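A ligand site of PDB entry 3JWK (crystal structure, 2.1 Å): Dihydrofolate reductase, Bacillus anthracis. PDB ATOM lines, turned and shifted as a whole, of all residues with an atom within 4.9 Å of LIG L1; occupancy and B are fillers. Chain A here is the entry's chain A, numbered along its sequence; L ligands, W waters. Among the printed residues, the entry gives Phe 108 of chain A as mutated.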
ATOM      1  N   MET A  12      20.948 -11.176 -14.134  1.00  0.00           N
ATOM      2  CA  MET A  12      21.730 -11.739 -15.217  1.00  0.00           C
ATOM      3  C   MET A  12      20.880 -12.777 -15.942  1.00  0.00           C
ATOM      4  O   MET A  12      20.501 -13.779 -15.358  1.00  0.00           O
ATOM      5  CB  MET A  12      23.032 -12.335 -14.674  1.00  0.00           C
ATOM      6  CG  MET A  12      23.828 -13.184 -15.679  1.00  0.00           C
ATOM      7  SD  MET A  12      24.578 -12.287 -17.042  1.00  0.00           S
ATOM      8  CE  MET A  12      25.817 -11.320 -16.158  1.00  0.00           C
ATOM      9  N   VAL A  13      20.564 -12.523 -17.216  1.00  0.00           N
ATOM     10  CA  VAL A  13      19.637 -13.360 -17.990  1.00  0.00           C
ATOM     11  C   VAL A  13      19.981 -13.389 -19.480  1.00  0.00           C
ATOM     12  O   VAL A  13      20.462 -12.419 -20.032  1.00  0.00           O
ATOM     13  CB  VAL A  13      18.142 -12.929 -17.759  1.00  0.00           C
ATOM     14  CG1 VAL A  13      17.865 -11.515 -18.238  1.00  0.00           C
ATOM     15  CG2 VAL A  13      17.159 -13.912 -18.405  1.00  0.00           C
ATOM     16  N   ALA A  14      19.745 -14.532 -20.120  1.00  0.00           N
ATOM     17  CA  ALA A  14      19.775 -14.622 -21.575  1.00  0.00           C
ATOM     18  C   ALA A  14      18.374 -15.019 -22.049  1.00  0.00           C
ATOM     19  O   ALA A  14      17.809 -16.004 -21.567  1.00  0.00           O
ATOM     20  CB  ALA A  14      20.815 -15.660 -22.037  1.00  0.00           C
ATOM     21  N   ILE A  21      13.454 -18.240 -21.817  1.00  0.00           N
ATOM     22  CA  ILE A  21      14.720 -18.511 -21.126  1.00  0.00           C
ATOM     23  C   ILE A  21      14.961 -20.004 -20.917  1.00  0.00           C
ATOM     24  O   ILE A  21      16.081 -20.410 -20.615  1.00  0.00           O
ATOM     25  CB  ILE A  21      14.868 -17.741 -19.780  1.00  0.00           C
ATOM     26  CG1 ILE A  21      13.798 -18.156 -18.743  1.00  0.00           C
ATOM     27  CG2 ILE A  21      14.854 -16.235 -20.016  1.00  0.00           C
ATOM     28  CD1 ILE A  21      14.061 -17.606 -17.320  1.00  0.00           C
ATOM     29  N   GLY A  22      13.921 -20.813 -21.107  1.00  0.00           N
ATOM     30  CA  GLY A  22      14.022 -22.248 -20.826  1.00  0.00           C
ATOM     31  C   GLY A  22      13.019 -23.127 -21.558  1.00  0.00           C
ATOM     32  O   GLY A  22      11.938 -22.679 -21.939  1.00  0.00           O
ATOM     33  N   LYS A  23      13.420 -24.377 -21.771  1.00  0.00           N
ATOM     34  CA  LYS A  23      12.565 -25.403 -22.357  1.00  0.00           C
ATOM     35  C   LYS A  23      12.885 -26.713 -21.631  1.00  0.00           C
ATOM     36  O   LYS A  23      14.058 -27.065 -21.476  1.00  0.00           O
ATOM     37  CB  LYS A  23      12.841 -25.545 -23.854  1.00  0.00           C
ATOM     38  CG  LYS A  23      11.939 -26.537 -24.612  1.00  0.00           C
ATOM     39  CD  LYS A  23      12.707 -27.802 -25.015  1.00  0.00           C
ATOM     40  CE  LYS A  23      13.234 -27.746 -26.461  1.00  0.00           C
ATOM     41  NZ  LYS A  23      12.251 -28.268 -27.478  1.00  0.00           N
ATOM     42  N   ASN A  25      12.993 -27.576 -18.496  1.00  0.00           N
ATOM     43  CA  ASN A  25      13.926 -27.358 -17.376  1.00  0.00           C
ATOM     44  C   ASN A  25      15.420 -27.330 -17.774  1.00  0.00           C
ATOM     45  O   ASN A  25      16.312 -27.685 -16.970  1.00  0.00           O
ATOM     46  CB  ASN A  25      13.655 -28.359 -16.245  1.00  0.00           C
ATOM     47  CG  ASN A  25      14.226 -27.901 -14.925  1.00  0.00           C
ATOM     48  OD1 ASN A  25      14.265 -26.699 -14.622  1.00  0.00           O
ATOM     49  ND2 ASN A  25      14.686 -28.858 -14.110  1.00  0.00           N
ATOM     50  N   ASN A  26      15.681 -26.900 -19.004  1.00  0.00           N
ATOM     51  CA  ASN A  26      17.022 -26.719 -19.542  1.00  0.00           C
ATOM     52  C   ASN A  26      17.087 -25.445 -20.380  1.00  0.00           C
ATOM     53  O   ASN A  26      16.038 -24.845 -20.676  1.00  0.00           O
ATOM     54  CB  ASN A  26      17.414 -27.934 -20.400  1.00  0.00           C
ATOM     55  CG  ASN A  26      17.797 -29.154 -19.570  1.00  0.00           C
ATOM     56  OD1 ASN A  26      18.679 -29.095 -18.709  1.00  0.00           O
ATOM     57  ND2 ASN A  26      17.126 -30.277 -19.836  1.00  0.00           N
ATOM     58  N   LEU A  27      18.285 -25.055 -20.769  1.00  0.00           N
ATOM     59  CA  LEU A  27      18.531 -23.941 -21.673  1.00  0.00           C
ATOM     60  C   LEU A  27      18.237 -24.397 -23.102  1.00  0.00           C
ATOM     61  O   LEU A  27      18.705 -25.468 -23.499  1.00  0.00           O
ATOM     62  CB  LEU A  27      20.001 -23.545 -21.527  1.00  0.00           C
ATOM     63  CG  LEU A  27      20.542 -22.123 -21.596  1.00  0.00           C
ATOM     64  CD1 LEU A  27      19.625 -21.096 -20.954  1.00  0.00           C
ATOM     65  CD2 LEU A  27      21.929 -22.135 -20.937  1.00  0.00           C
ATOM     66  N   TRP A  29      19.414 -23.321 -25.896  1.00  0.00           N
ATOM     67  CA  TRP A  29      20.519 -23.065 -26.812  1.00  0.00           C
ATOM     68  C   TRP A  29      21.863 -23.368 -26.166  1.00  0.00           C
ATOM     69  O   TRP A  29      21.975 -23.395 -24.938  1.00  0.00           O
ATOM     70  CB  TRP A  29      20.514 -21.592 -27.258  1.00  0.00           C
ATOM     71  CG  TRP A  29      20.449 -20.643 -26.084  1.00  0.00           C
ATOM     72  CD1 TRP A  29      21.482 -20.269 -25.290  1.00  0.00           C
ATOM     73  CD2 TRP A  29      19.276 -19.976 -25.580  1.00  0.00           C
ATOM     74  NE1 TRP A  29      21.031 -19.411 -24.312  1.00  0.00           N
ATOM     75  CE2 TRP A  29      19.685 -19.216 -24.463  1.00  0.00           C
ATOM     76  CE3 TRP A  29      17.926 -19.940 -25.963  1.00  0.00           C
ATOM     77  CZ2 TRP A  29      18.791 -18.430 -23.720  1.00  0.00           C
ATOM     78  CZ3 TRP A  29      17.026 -19.160 -25.216  1.00  0.00           C
ATOM     79  CH2 TRP A  29      17.477 -18.427 -24.107  1.00  0.00           C
ATOM     80  N   GLY A  50      17.157 -19.900  -8.146  1.00  0.00           N
ATOM     81  CA  GLY A  50      16.025 -20.722  -7.715  1.00  0.00           C
ATOM     82  C   GLY A  50      16.472 -22.164  -7.614  1.00  0.00           C
ATOM     83  O   GLY A  50      17.414 -22.574  -8.272  1.00  0.00           O
ATOM     84  N   ARG A  51      15.786 -22.935  -6.772  1.00  0.00           N
ATOM     85  CA  ARG A  51      16.181 -24.321  -6.526  1.00  0.00           C
ATOM     86  C   ARG A  51      16.270 -25.139  -7.832  1.00  0.00           C
ATOM     87  O   ARG A  51      17.182 -25.931  -8.000  1.00  0.00           O
ATOM     88  CB  ARG A  51      15.244 -24.974  -5.509  1.00  0.00           C
ATOM     89  CG  ARG A  51      15.726 -26.298  -4.931  1.00  0.00           C
ATOM     90  CD  ARG A  51      15.134 -27.503  -5.684  1.00  0.00           C
ATOM     91  NE  ARG A  51      13.670 -27.453  -5.733  1.00  0.00           N
ATOM     92  CZ  ARG A  51      12.935 -28.157  -6.583  1.00  0.00           C
ATOM     93  NH1 ARG A  51      13.513 -28.960  -7.475  1.00  0.00           N
ATOM     94  NH2 ARG A  51      11.614 -28.044  -6.559  1.00  0.00           N
ATOM     95  N   LYS A  52      15.329 -24.924  -8.759  1.00  0.00           N
ATOM     96  CA  LYS A  52      15.319 -25.692 -10.021  1.00  0.00           C
ATOM     97  C   LYS A  52      16.477 -25.341 -10.938  1.00  0.00           C
ATOM     98  O   LYS A  52      17.130 -26.227 -11.499  1.00  0.00           O
ATOM     99  CB  LYS A  52      13.985 -25.533 -10.749  1.00  0.00           C
ATOM    100  CG  LYS A  52      12.858 -26.318 -10.105  1.00  0.00           C
ATOM    101  CD  LYS A  52      11.716 -26.557 -11.088  1.00  0.00           C
ATOM    102  CE  LYS A  52      10.393 -26.749 -10.355  1.00  0.00           C
ATOM    103  NZ  LYS A  52       9.264 -26.940 -11.332  1.00  0.00           N
ATOM    104  N   ASN A  53      16.738 -24.033 -11.083  1.00  0.00           N
ATOM    105  CA  ASN A  53      17.944 -23.561 -11.767  1.00  0.00           C
ATOM    106  C   ASN A  53      19.197 -24.233 -11.177  1.00  0.00           C
ATOM    107  O   ASN A  53      19.985 -24.817 -11.926  1.00  0.00           O
ATOM    108  CB  ASN A  53      18.050 -22.029 -11.660  1.00  0.00           C
ATOM    109  CG  ASN A  53      19.340 -21.456 -12.299  1.00  0.00           C
ATOM    110  OD1 ASN A  53      19.954 -22.085 -13.143  1.00  0.00           O
ATOM    111  ND2 ASN A  53      19.704 -20.251 -11.890  1.00  0.00           N
ATOM    112  N   VAL A  69      17.549 -20.502  -3.503  1.00  0.00           N
ATOM    113  CA  VAL A  69      16.260 -20.086  -2.943  1.00  0.00           C
ATOM    114  C   VAL A  69      15.226 -21.201  -3.055  1.00  0.00           C
ATOM    115  O   VAL A  69      14.942 -21.684  -4.156  1.00  0.00           O
ATOM    116  CB  VAL A  69      15.736 -18.760  -3.565  1.00  0.00           C
ATOM    117  CG1 VAL A  69      14.454 -18.298  -2.861  1.00  0.00           C
ATOM    118  CG2 VAL A  69      16.796 -17.680  -3.447  1.00  0.00           C
ATOM    119  N   THR A  70      14.679 -21.588  -1.907  1.00  0.00           N
ATOM    120  CA  THR A  70      13.725 -22.696  -1.791  1.00  0.00           C
ATOM    121  C   THR A  70      12.762 -22.416  -0.629  1.00  0.00           C
ATOM    122  O   THR A  70      13.084 -21.669   0.293  1.00  0.00           O
ATOM    123  CB  THR A  70      14.444 -24.064  -1.563  1.00  0.00           C
ATOM    124  OG1 THR A  70      13.486 -25.108  -1.344  1.00  0.00           O
ATOM    125  CG2 THR A  70      15.378 -24.025  -0.340  1.00  0.00           C
ATOM    126  N   ARG A  71      11.571 -22.994  -0.697  1.00  0.00           N
ATOM    127  CA  ARG A  71      10.628 -22.910   0.412  1.00  0.00           C
ATOM    128  C   ARG A  71      10.880 -24.047   1.417  1.00  0.00           C
ATOM    129  O   ARG A  71      10.316 -24.064   2.508  1.00  0.00           O
ATOM    130  CB  ARG A  71       9.196 -22.966  -0.115  1.00  0.00           C
ATOM    131  CG  ARG A  71       8.799 -21.750  -0.918  1.00  0.00           C
ATOM    132  CD  ARG A  71       7.312 -21.735  -1.147  1.00  0.00           C
ATOM    133  NE  ARG A  71       6.867 -20.596  -1.934  1.00  0.00           N
ATOM    134  CZ  ARG A  71       6.782 -20.585  -3.268  1.00  0.00           C
ATOM    135  NH1 ARG A  71       7.123 -21.668  -3.965  1.00  0.00           N
ATOM    136  NH2 ARG A  71       6.351 -19.499  -3.900  1.00  0.00           N
ATOM    137  N   ASN A  72      11.746 -24.980   1.005  1.00  0.00           N
ATOM    138  CA  ASN A  72      12.069 -26.176   1.773  1.00  0.00           C
ATOM    139  C   ASN A  72      13.006 -25.819   2.928  1.00  0.00           C
ATOM    140  O   ASN A  72      14.180 -25.569   2.711  1.00  0.00           O
ATOM    141  CB  ASN A  72      12.722 -27.199   0.823  1.00  0.00           C
ATOM    142  CG  ASN A  72      12.887 -28.586   1.423  1.00  0.00           C
ATOM    143  OD1 ASN A  72      13.003 -29.563   0.681  1.00  0.00           O
ATOM    144  ND2 ASN A  72      12.923 -28.698   2.750  1.00  0.00           N
ATOM    145  N   HIS A  84      15.326 -18.727   2.063  1.00  0.00           N
ATOM    146  CA  HIS A  84      13.937 -19.119   1.869  1.00  0.00           C
ATOM    147  C   HIS A  84      13.013 -17.952   1.545  1.00  0.00           C
ATOM    148  O   HIS A  84      11.806 -18.137   1.414  1.00  0.00           O
ATOM    149  CB  HIS A  84      13.431 -19.922   3.074  1.00  0.00           C
ATOM    150  CG  HIS A  84      14.345 -21.046   3.441  1.00  0.00           C
ATOM    151  ND1 HIS A  84      15.359 -20.905   4.365  1.00  0.00           N
ATOM    152  CD2 HIS A  84      14.419 -22.319   2.985  1.00  0.00           C
ATOM    153  CE1 HIS A  84      16.013 -22.050   4.467  1.00  0.00           C
ATOM    154  NE2 HIS A  84      15.462 -22.929   3.645  1.00  0.00           N
ATOM    155  N   SER A  85      13.604 -16.769   1.391  1.00  0.00           N
ATOM    156  CA  SER A  85      12.841 -15.551   1.117  1.00  0.00           C
ATOM    157  C   SER A  85      13.754 -14.447   0.576  1.00  0.00           C
ATOM    158  O   SER A  85      14.979 -14.545   0.679  1.00  0.00           O
ATOM    159  CB  SER A  85      12.130 -15.059   2.393  1.00  0.00           C
ATOM    160  OG  SER A  85      13.061 -14.599   3.363  1.00  0.00           O
ATOM    161  N   PHE A 102      20.113 -14.836 -10.774  1.00  0.00           N
ATOM    162  CA  PHE A 102      20.657 -15.689 -11.839  1.00  0.00           C
ATOM    163  C   PHE A 102      19.562 -16.583 -12.444  1.00  0.00           C
ATOM    164  O   PHE A 102      19.830 -17.348 -13.381  1.00  0.00           O
ATOM    165  CB  PHE A 102      21.786 -16.538 -11.227  1.00  0.00           C
ATOM    166  CG  PHE A 102      22.845 -17.001 -12.207  1.00  0.00           C
ATOM    167  CD1 PHE A 102      23.521 -16.111 -13.022  1.00  0.00           C
ATOM    168  CD2 PHE A 102      23.205 -18.345 -12.243  1.00  0.00           C
ATOM    169  CE1 PHE A 102      24.512 -16.551 -13.898  1.00  0.00           C
ATOM    170  CE2 PHE A 102      24.194 -18.809 -13.112  1.00  0.00           C
ATOM    171  CZ  PHE A 102      24.858 -17.899 -13.937  1.00  0.00           C
ATOM    172  N   GLY A 103      18.335 -16.468 -11.930  1.00  0.00           N
ATOM    173  CA  GLY A 103      17.192 -17.250 -12.444  1.00  0.00           C
ATOM    174  C   GLY A 103      16.863 -18.509 -11.647  1.00  0.00           C
ATOM    175  O   GLY A 103      17.535 -18.808 -10.650  1.00  0.00           O
ATOM    176  N   GLY A 104      15.850 -19.277 -12.065  1.00  0.00           N
ATOM    177  CA  GLY A 104      15.088 -19.029 -13.284  1.00  0.00           C
ATOM    178  C   GLY A 104      13.907 -18.084 -13.112  1.00  0.00           C
ATOM    179  O   GLY A 104      13.982 -17.131 -12.334  1.00  0.00           O
ATOM    180  N   ALA A 105      12.837 -18.356 -13.845  1.00  0.00           N
ATOM    181  CA  ALA A 105      11.734 -17.410 -13.981  1.00  0.00           C
ATOM    182  C   ALA A 105      11.052 -17.055 -12.641  1.00  0.00           C
ATOM    183  O   ALA A 105      10.771 -15.892 -12.390  1.00  0.00           O
ATOM    184  CB  ALA A 105      10.727 -17.916 -14.982  1.00  0.00           C
ATOM    185  N   GLN A 106      10.802 -18.056 -11.806  1.00  0.00           N
ATOM    186  CA  GLN A 106      10.172 -17.814 -10.490  1.00  0.00           C
ATOM    187  C   GLN A 106      11.034 -16.897  -9.636  1.00  0.00           C
ATOM    188  O   GLN A 106      10.527 -16.031  -8.933  1.00  0.00           O
ATOM    189  CB  GLN A 106       9.955 -19.119  -9.733  1.00  0.00           C
ATOM    190  CG  GLN A 106       8.945 -20.057 -10.365  1.00  0.00           C
ATOM    191  CD  GLN A 106       8.505 -21.144  -9.407  1.00  0.00           C
ATOM    192  OE1 GLN A 106       8.485 -22.325  -9.750  1.00  0.00           O
ATOM    193  NE2 GLN A 106       8.151 -20.759  -8.202  1.00  0.00           N
ATOM    194  N   ILE A 107      12.344 -17.112  -9.689  1.00  0.00           N
ATOM    195  CA  ILE A 107      13.275 -16.281  -8.921  1.00  0.00           C
ATOM    196  C   ILE A 107      13.438 -14.881  -9.545  1.00  0.00           C
ATOM    197  O   ILE A 107      13.545 -13.894  -8.813  1.00  0.00           O
ATOM    198  CB  ILE A 107      14.614 -17.042  -8.638  1.00  0.00           C
ATOM    199  CG1 ILE A 107      14.629 -17.608  -7.209  1.00  0.00           C
ATOM    200  CG2 ILE A 107      15.809 -16.133  -8.792  1.00  0.00           C
ATOM    201  CD1 ILE A 107      13.447 -18.511  -6.805  1.00  0.00           C
ATOM    202  N   PHE A 108      13.402 -14.770 -10.872  1.00  0.00           N
ATOM    203  CA  PHE A 108      13.362 -13.433 -11.497  1.00  0.00           C
ATOM    204  C   PHE A 108      12.077 -12.663 -11.105  1.00  0.00           C
ATOM    205  O   PHE A 108      12.153 -11.461 -10.794  1.00  0.00           O
ATOM    206  CB  PHE A 108      13.463 -13.519 -13.020  1.00  0.00           C
ATOM    207  CG  PHE A 108      14.832 -13.894 -13.556  1.00  0.00           C
ATOM    208  CD1 PHE A 108      14.936 -14.853 -14.556  1.00  0.00           C
ATOM    209  CD2 PHE A 108      15.992 -13.268 -13.105  1.00  0.00           C
ATOM    210  CE1 PHE A 108      16.183 -15.208 -15.095  1.00  0.00           C
ATOM    211  CE2 PHE A 108      17.234 -13.617 -13.639  1.00  0.00           C
ATOM    212  CZ  PHE A 108      17.328 -14.576 -14.629  1.00  0.00           C
ATOM    213  N   LEU A 110      10.337 -13.094  -8.380  1.00  0.00           N
ATOM    214  CA  LEU A 110      10.502 -12.822  -6.955  1.00  0.00           C
ATOM    215  C   LEU A 110      11.252 -11.509  -6.677  1.00  0.00           C
ATOM    216  O   LEU A 110      10.802 -10.691  -5.875  1.00  0.00           O
ATOM    217  CB  LEU A 110      11.227 -13.999  -6.296  1.00  0.00           C
ATOM    218  CG  LEU A 110      11.220 -14.140  -4.780  1.00  0.00           C
ATOM    219  CD1 LEU A 110       9.815 -13.870  -4.177  1.00  0.00           C
ATOM    220  CD2 LEU A 110      11.725 -15.523  -4.408  1.00  0.00           C
ATOM    221  N   THR A 131       9.420 -21.498 -20.404  1.00  0.00           N
ATOM    222  CA  THR A 131       9.801 -20.631 -19.290  1.00  0.00           C
ATOM    223  C   THR A 131      10.258 -19.264 -19.821  1.00  0.00           C
ATOM    224  O   THR A 131      11.034 -19.187 -20.777  1.00  0.00           O
ATOM    225  CB  THR A 131      10.901 -21.317 -18.441  1.00  0.00           C
ATOM    226  OG1 THR A 131      10.478 -22.655 -18.119  1.00  0.00           O
ATOM    227  CG2 THR A 131      11.172 -20.568 -17.120  1.00  0.00           C
HETATM  228  P1  LIG L   1      13.487 -21.477 -10.644  1.00  0.00           P
HETATM  229  O1  LIG L   1      12.948 -20.103 -10.580  1.00  0.00           O
HETATM  230  O2  LIG L   1      14.915 -21.567 -10.996  1.00  0.00           O
HETATM  231  O3  LIG L   1      13.230 -22.256  -9.279  1.00  0.00           O
HETATM  232  C1  LIG L   1      11.924 -22.553  -8.865  1.00  0.00           C
HETATM  233  C2  LIG L   1      12.035 -22.873  -7.389  1.00  0.00           C
HETATM  234  O4  LIG L   1      12.449 -21.726  -6.675  1.00  0.00           O
HETATM  235  C3  LIG L   1      10.709 -23.282  -6.767  1.00  0.00           C
HETATM  236  O5  LIG L   1      10.420 -24.624  -7.085  1.00  0.00           O
HETATM  237  C4  LIG L   1      11.024 -23.029  -5.308  1.00  0.00           C
HETATM  238  O6  LIG L   1      11.814 -24.082  -4.779  1.00  0.00           O
HETATM  239  C5  LIG L   1      11.881 -21.760  -5.383  1.00  0.00           C
HETATM  240  N1  LIG L   1      10.987 -20.618  -5.152  1.00  0.00           N
HETATM  241  C6  LIG L   1      10.122 -20.018  -6.046  1.00  0.00           C
HETATM  242  N2  LIG L   1       9.459 -19.022  -5.416  1.00  0.00           N
HETATM  243  C7  LIG L   1       9.885 -18.973  -4.131  1.00  0.00           C
HETATM  244  C8  LIG L   1       9.562 -18.167  -3.052  1.00  0.00           C
HETATM  245  N3  LIG L   1       8.654 -17.199  -3.166  1.00  0.00           N
HETATM  246  N4  LIG L   1      10.184 -18.372  -1.854  1.00  0.00           N
HETATM  247  C9  LIG L   1      11.129 -19.350  -1.692  1.00  0.00           C
HETATM  248  N5  LIG L   1      11.447 -20.150  -2.765  1.00  0.00           N
HETATM  249  C10 LIG L   1      10.841 -19.970  -3.959  1.00  0.00           C
HETATM  250  O7  LIG L   1      12.572 -22.344 -11.644  1.00  0.00           O
HETATM  251  P2  LIG L   1      11.887 -22.037 -13.046  1.00  0.00           P
HETATM  252  O8  LIG L   1      11.262 -23.310 -13.488  1.00  0.00           O
HETATM  253  O9  LIG L   1      11.112 -20.774 -12.970  1.00  0.00           O
HETATM  254  O10 LIG L   1      13.195 -21.751 -13.973  1.00  0.00           O
HETATM  255  C11 LIG L   1      13.951 -22.838 -14.469  1.00  0.00           C
HETATM  256  C12 LIG L   1      14.130 -22.714 -15.970  1.00  0.00           C
HETATM  257  O11 LIG L   1      14.734 -21.469 -16.272  1.00  0.00           O
HETATM  258  C13 LIG L   1      15.041 -23.777 -16.548  1.00  0.00           C
HETATM  259  O12 LIG L   1      14.575 -24.089 -17.841  1.00  0.00           O
HETATM  260  C14 LIG L   1      16.382 -23.078 -16.694  1.00  0.00           C
HETATM  261  O13 LIG L   1      17.129 -23.637 -17.742  1.00  0.00           O
HETATM  262  C15 LIG L   1      15.915 -21.682 -17.055  1.00  0.00           C
HETATM  263  N6  LIG L   1      16.912 -20.624 -16.770  1.00  0.00           N
HETATM  264  C16 LIG L   1      17.312 -19.849 -17.811  1.00  0.00           C
HETATM  265  C17 LIG L   1      18.233 -18.818 -17.607  1.00  0.00           C
HETATM  266  C18 LIG L   1      18.545 -17.911 -18.742  1.00  0.00           C
HETATM  267  O14 LIG L   1      19.149 -16.692 -18.460  1.00  0.00           O
HETATM  268  N7  LIG L   1      18.265 -18.255 -19.996  1.00  0.00           N
HETATM  269  C19 LIG L   1      18.738 -18.570 -16.319  1.00  0.00           C
HETATM  270  C20 LIG L   1      18.307 -19.380 -15.262  1.00  0.00           C
HETATM  271  C21 LIG L   1      17.399 -20.407 -15.492  1.00  0.00           C
HETATM  272  P3  LIG L   1      11.232 -25.330  -3.950  1.00  0.00           P
HETATM  273  O15 LIG L   1      10.443 -24.792  -2.783  1.00  0.00           O
HETATM  274  O16 LIG L   1      10.351 -26.133  -4.900  1.00  0.00           O
HETATM  275  O17 LIG L   1      12.399 -26.155  -3.524  1.00  0.00           O
HETATM  276  N1  LG2 L   2      23.267 -16.557 -19.499  1.00  0.00           N
HETATM  277  C1  LG2 L   2      22.920 -15.380 -18.946  1.00  0.00           C
HETATM  278  N2  LG2 L   2      22.374 -15.328 -17.729  1.00  0.00           N
HETATM  279  C2  LG2 L   2      22.152 -16.466 -17.017  1.00  0.00           C
HETATM  280  C3  LG2 L   2      22.503 -17.693 -17.579  1.00  0.00           C
HETATM  281  C4  LG2 L   2      23.074 -17.707 -18.850  1.00  0.00           C
HETATM  282  C5  LG2 L   2      27.095 -20.816 -15.807  1.00  0.00           C
HETATM  283  C6  LG2 L   2      22.210 -25.978 -17.008  1.00  0.00           C
HETATM  284  C7  LG2 L   2      27.226 -24.997 -15.937  1.00  0.00           C
HETATM  285  C8  LG2 L   2      20.383 -22.039 -17.367  1.00  0.00           C
HETATM  286  C9  LG2 L   2      23.480 -19.038 -19.505  1.00  0.00           C
HETATM  287  N3  LG2 L   2      23.143 -14.262 -19.637  1.00  0.00           N
HETATM  288  N4  LG2 L   2      21.594 -16.418 -15.803  1.00  0.00           N
HETATM  289  C10 LG2 L   2      22.301 -18.916 -16.863  1.00  0.00           C
HETATM  290  C11 LG2 L   2      22.136 -19.962 -16.301  1.00  0.00           C
HETATM  291  C12 LG2 L   2      24.486 -21.734 -15.891  1.00  0.00           C
HETATM  292  C13 LG2 L   2      22.906 -23.454 -16.463  1.00  0.00           C
HETATM  293  O1  LG2 L   2      26.857 -22.188 -16.157  1.00  0.00           O
HETATM  294  O2  LG2 L   2      23.598 -25.587 -17.248  1.00  0.00           O
HETATM  295  O3  LG2 L   2      26.298 -24.720 -17.041  1.00  0.00           O
HETATM  296  O4  LG2 L   2      20.718 -21.982 -15.961  1.00  0.00           O
HETATM  297  C14 LG2 L   2      23.162 -22.166 -16.019  1.00  0.00           C
HETATM  298  C15 LG2 L   2      25.542 -22.585 -16.251  1.00  0.00           C
HETATM  299  C16 LG2 L   2      23.926 -24.324 -16.811  1.00  0.00           C
HETATM  300  C17 LG2 L   2      25.260 -23.882 -16.703  1.00  0.00           C
HETATM  301  C18 LG2 L   2      21.966 -21.281 -15.639  1.00  0.00           C
HETATM  302  O   HOH W   1       9.261 -23.874 -11.705  1.00  0.00           O
HETATM  303  O   HOH W   2       9.079 -16.486   0.207  1.00  0.00           O
HETATM  304  O   HOH W   3       7.800 -24.240  -3.343  1.00  0.00           O
HETATM  305  O   HOH W   4      11.586 -25.294 -18.508  1.00  0.00           O
HETATM  306  O   HOH W   5      18.553 -25.462 -16.336  1.00  0.00           O
HETATM  307  O   HOH W   6      16.647 -25.630 -14.273  1.00  0.00           O
HETATM  308  O   HOH W   7       7.356 -17.569  -6.018  1.00  0.00           O
HETATM  309  O   HOH W   8      12.411 -28.571  -2.513  1.00  0.00           O
HETATM  310  O   HOH W   9       8.438 -27.783  -4.759  1.00  0.00           O
HETATM  311  O   HOH W  10      11.674 -25.323 -15.156  1.00  0.00           O
HETATM  312  O   HOH W  11       8.675 -20.690 -14.248  1.00  0.00           O
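OG1 of Thr 70 sits at hydrogen-bond distance from O17 of LIG L1 (2.7 Å). The backbone NH of Gly 104 sits at hydrogen-bond distance from an oxygen (O2) of LIG L1 (2.7 Å). The backbone NH (N) of Ala 14 lies within hydrogen-bond range of an oxygen (O14) of LIG L1 (2.8 Å). The backbone carbonyl oxygen (O) of Ala 14 is in hydrogen-bond range of a nitrogen (N7) of LIG L1, 2.8 Å away. O16 of LIG L1 is in salt-bridge range of NH2 of Arg 51 (2.8 Å). O9 of LIG L1 is in hydrogen-bond range of N of Gln 106, at 3.0 Å. An oxygen (O15) of LIG L1 is in hydrogen-bond range of the backbone NH of Arg 71. NH2 of Arg 71 is in hydrogen-bond range of N2 of LIG L1, 3.5 Å away. An oxygen (O2) of LIG L1 is in hydrogen-bond range of the backbone NH (N) of Asn 53. N of Ala 105 sits at hydrogen-bond distance from O9 of LIG L1 (3.1 Å). A nitrogen (N7) of LIG L1 lies close to the backbone carbonyl oxygen (O) of Ile 21, 3.1 Å away. An oxygen (O1) of LIG L1 is in hydrogen-bond range of the backbone NH of Ile 107 (3.2 Å). An oxygen (O12) of LIG L1 sits at hydrogen-bond distance from the backbone NH (N) of Asn 26. An oxygen (O12) of LIG L1 lies within hydrogen-bond range of the backbone carbonyl oxygen (O) of Asn 26 (3.3 Å). An oxygen (O3) of LIG L1 is in hydrogen-bond range of the backbone NH (N) of Lys 52, at 3.4 Å. The side-chain amide oxygen (OD1) of Asn 53 lies close to an oxygen (O4) of LG2 L2, at 2.9 Å. The backbone carbonyl oxygen (O) of Phe 102 lies within hydrogen-bond range of a nitrogen (N4) of LG2 L2 (3.1 Å). N of Val 13 lies within hydrogen-bond range of N2 of LG2 L2, 3.4 Å away. O of Val 13 is in hydrogen-bond range of N3 of LG2 L2 (3.3 Å). O of Met 12 sits at hydrogen-bond distance from N4 of LG2 L2 (2.9 Å). The side-chain sulfur (SD) of Met 12 sits at hydrogen-bond distance from a nitrogen (N3) of LG2 L2 (3.6 Å).
The backbone NH (N) of Asn 72 sits at hydrogen-bond distance from the side-chain hydroxyl (OG1) of Thr 70, at 2.9 Å. The backbone carbonyl oxygen of Val 69 sits at hydrogen-bond distance from the backbone NH of Arg 51 (3.0 Å). The side-chain amide nitrogen (ND2) of Asn 53 is in hydrogen-bond range of the backbone carbonyl oxygen (O) of Phe 102 (3.3 Å). The side-chain amide nitrogen (ND2) of Asn 53 sits at hydrogen-bond distance from the backbone carbonyl oxygen (O) of Gly 103 (2.9 Å). N of Ile 21 lies within hydrogen-bond range of O of Thr 131 (2.8 Å). NE2 of His 84 is in hydrogen-bond range of O of Asn 72 (3.1 Å). The backbone NH (N) of Gly 50 lies within hydrogen-bond range of the backbone carbonyl oxygen (O) of Gly 103 (2.8 Å). O of Gly 22 lies within hydrogen-bond range of N of Thr 131 (3.2 Å).
Residues that only touch LIG L1: Phe 102, Leu 27, Val 69, Asn 25, Val 13, His 84, Gly 22, Gly 50, Leu 110, Gly 103, Trp 29 and Thr 131. 24 residues have an atom within 4 Å of LIG L1: Val 13, Ala 14, Ile 21, Gly 22, Asn 25, Asn 26, Leu 27, Trp 29, Gly 50, Arg 51, Lys 52, Asn 53, Val 69, Thr 70, Arg 71, His 84, Phe 102, Gly 103, Gly 104, Ala 105, Gln 106, Ile 107, Leu 110 and Thr 131. The nearest printed residue that does not touch LIG L1 is Asn 72 (4.01 Å).
Water W8 bridges an oxygen (O17) of LIG L1 and the side-chain amide oxygen of Asn 72. Water W7 lies within hydrogen-bond range of N2 of LIG L1 and NH2 of Arg 71. Water W10 bridges O8 of LIG L1 (2.6 Å) and OD1 of Asn 25 (3.0 Å). Water W5 lies within hydrogen-bond range of an oxygen (O13) of LIG L1 and the backbone carbonyl oxygen (O) of Asn 25. Water W2 lies within hydrogen-bond range of a nitrogen (N4) of LIG L1 (3.0 Å) and the backbone carbonyl oxygen (O) of His 84 (3.4 Å). Water W6 bridges OD1 of Asn 25 (2.6 Å) and O of Lys 52 (2.9 Å).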
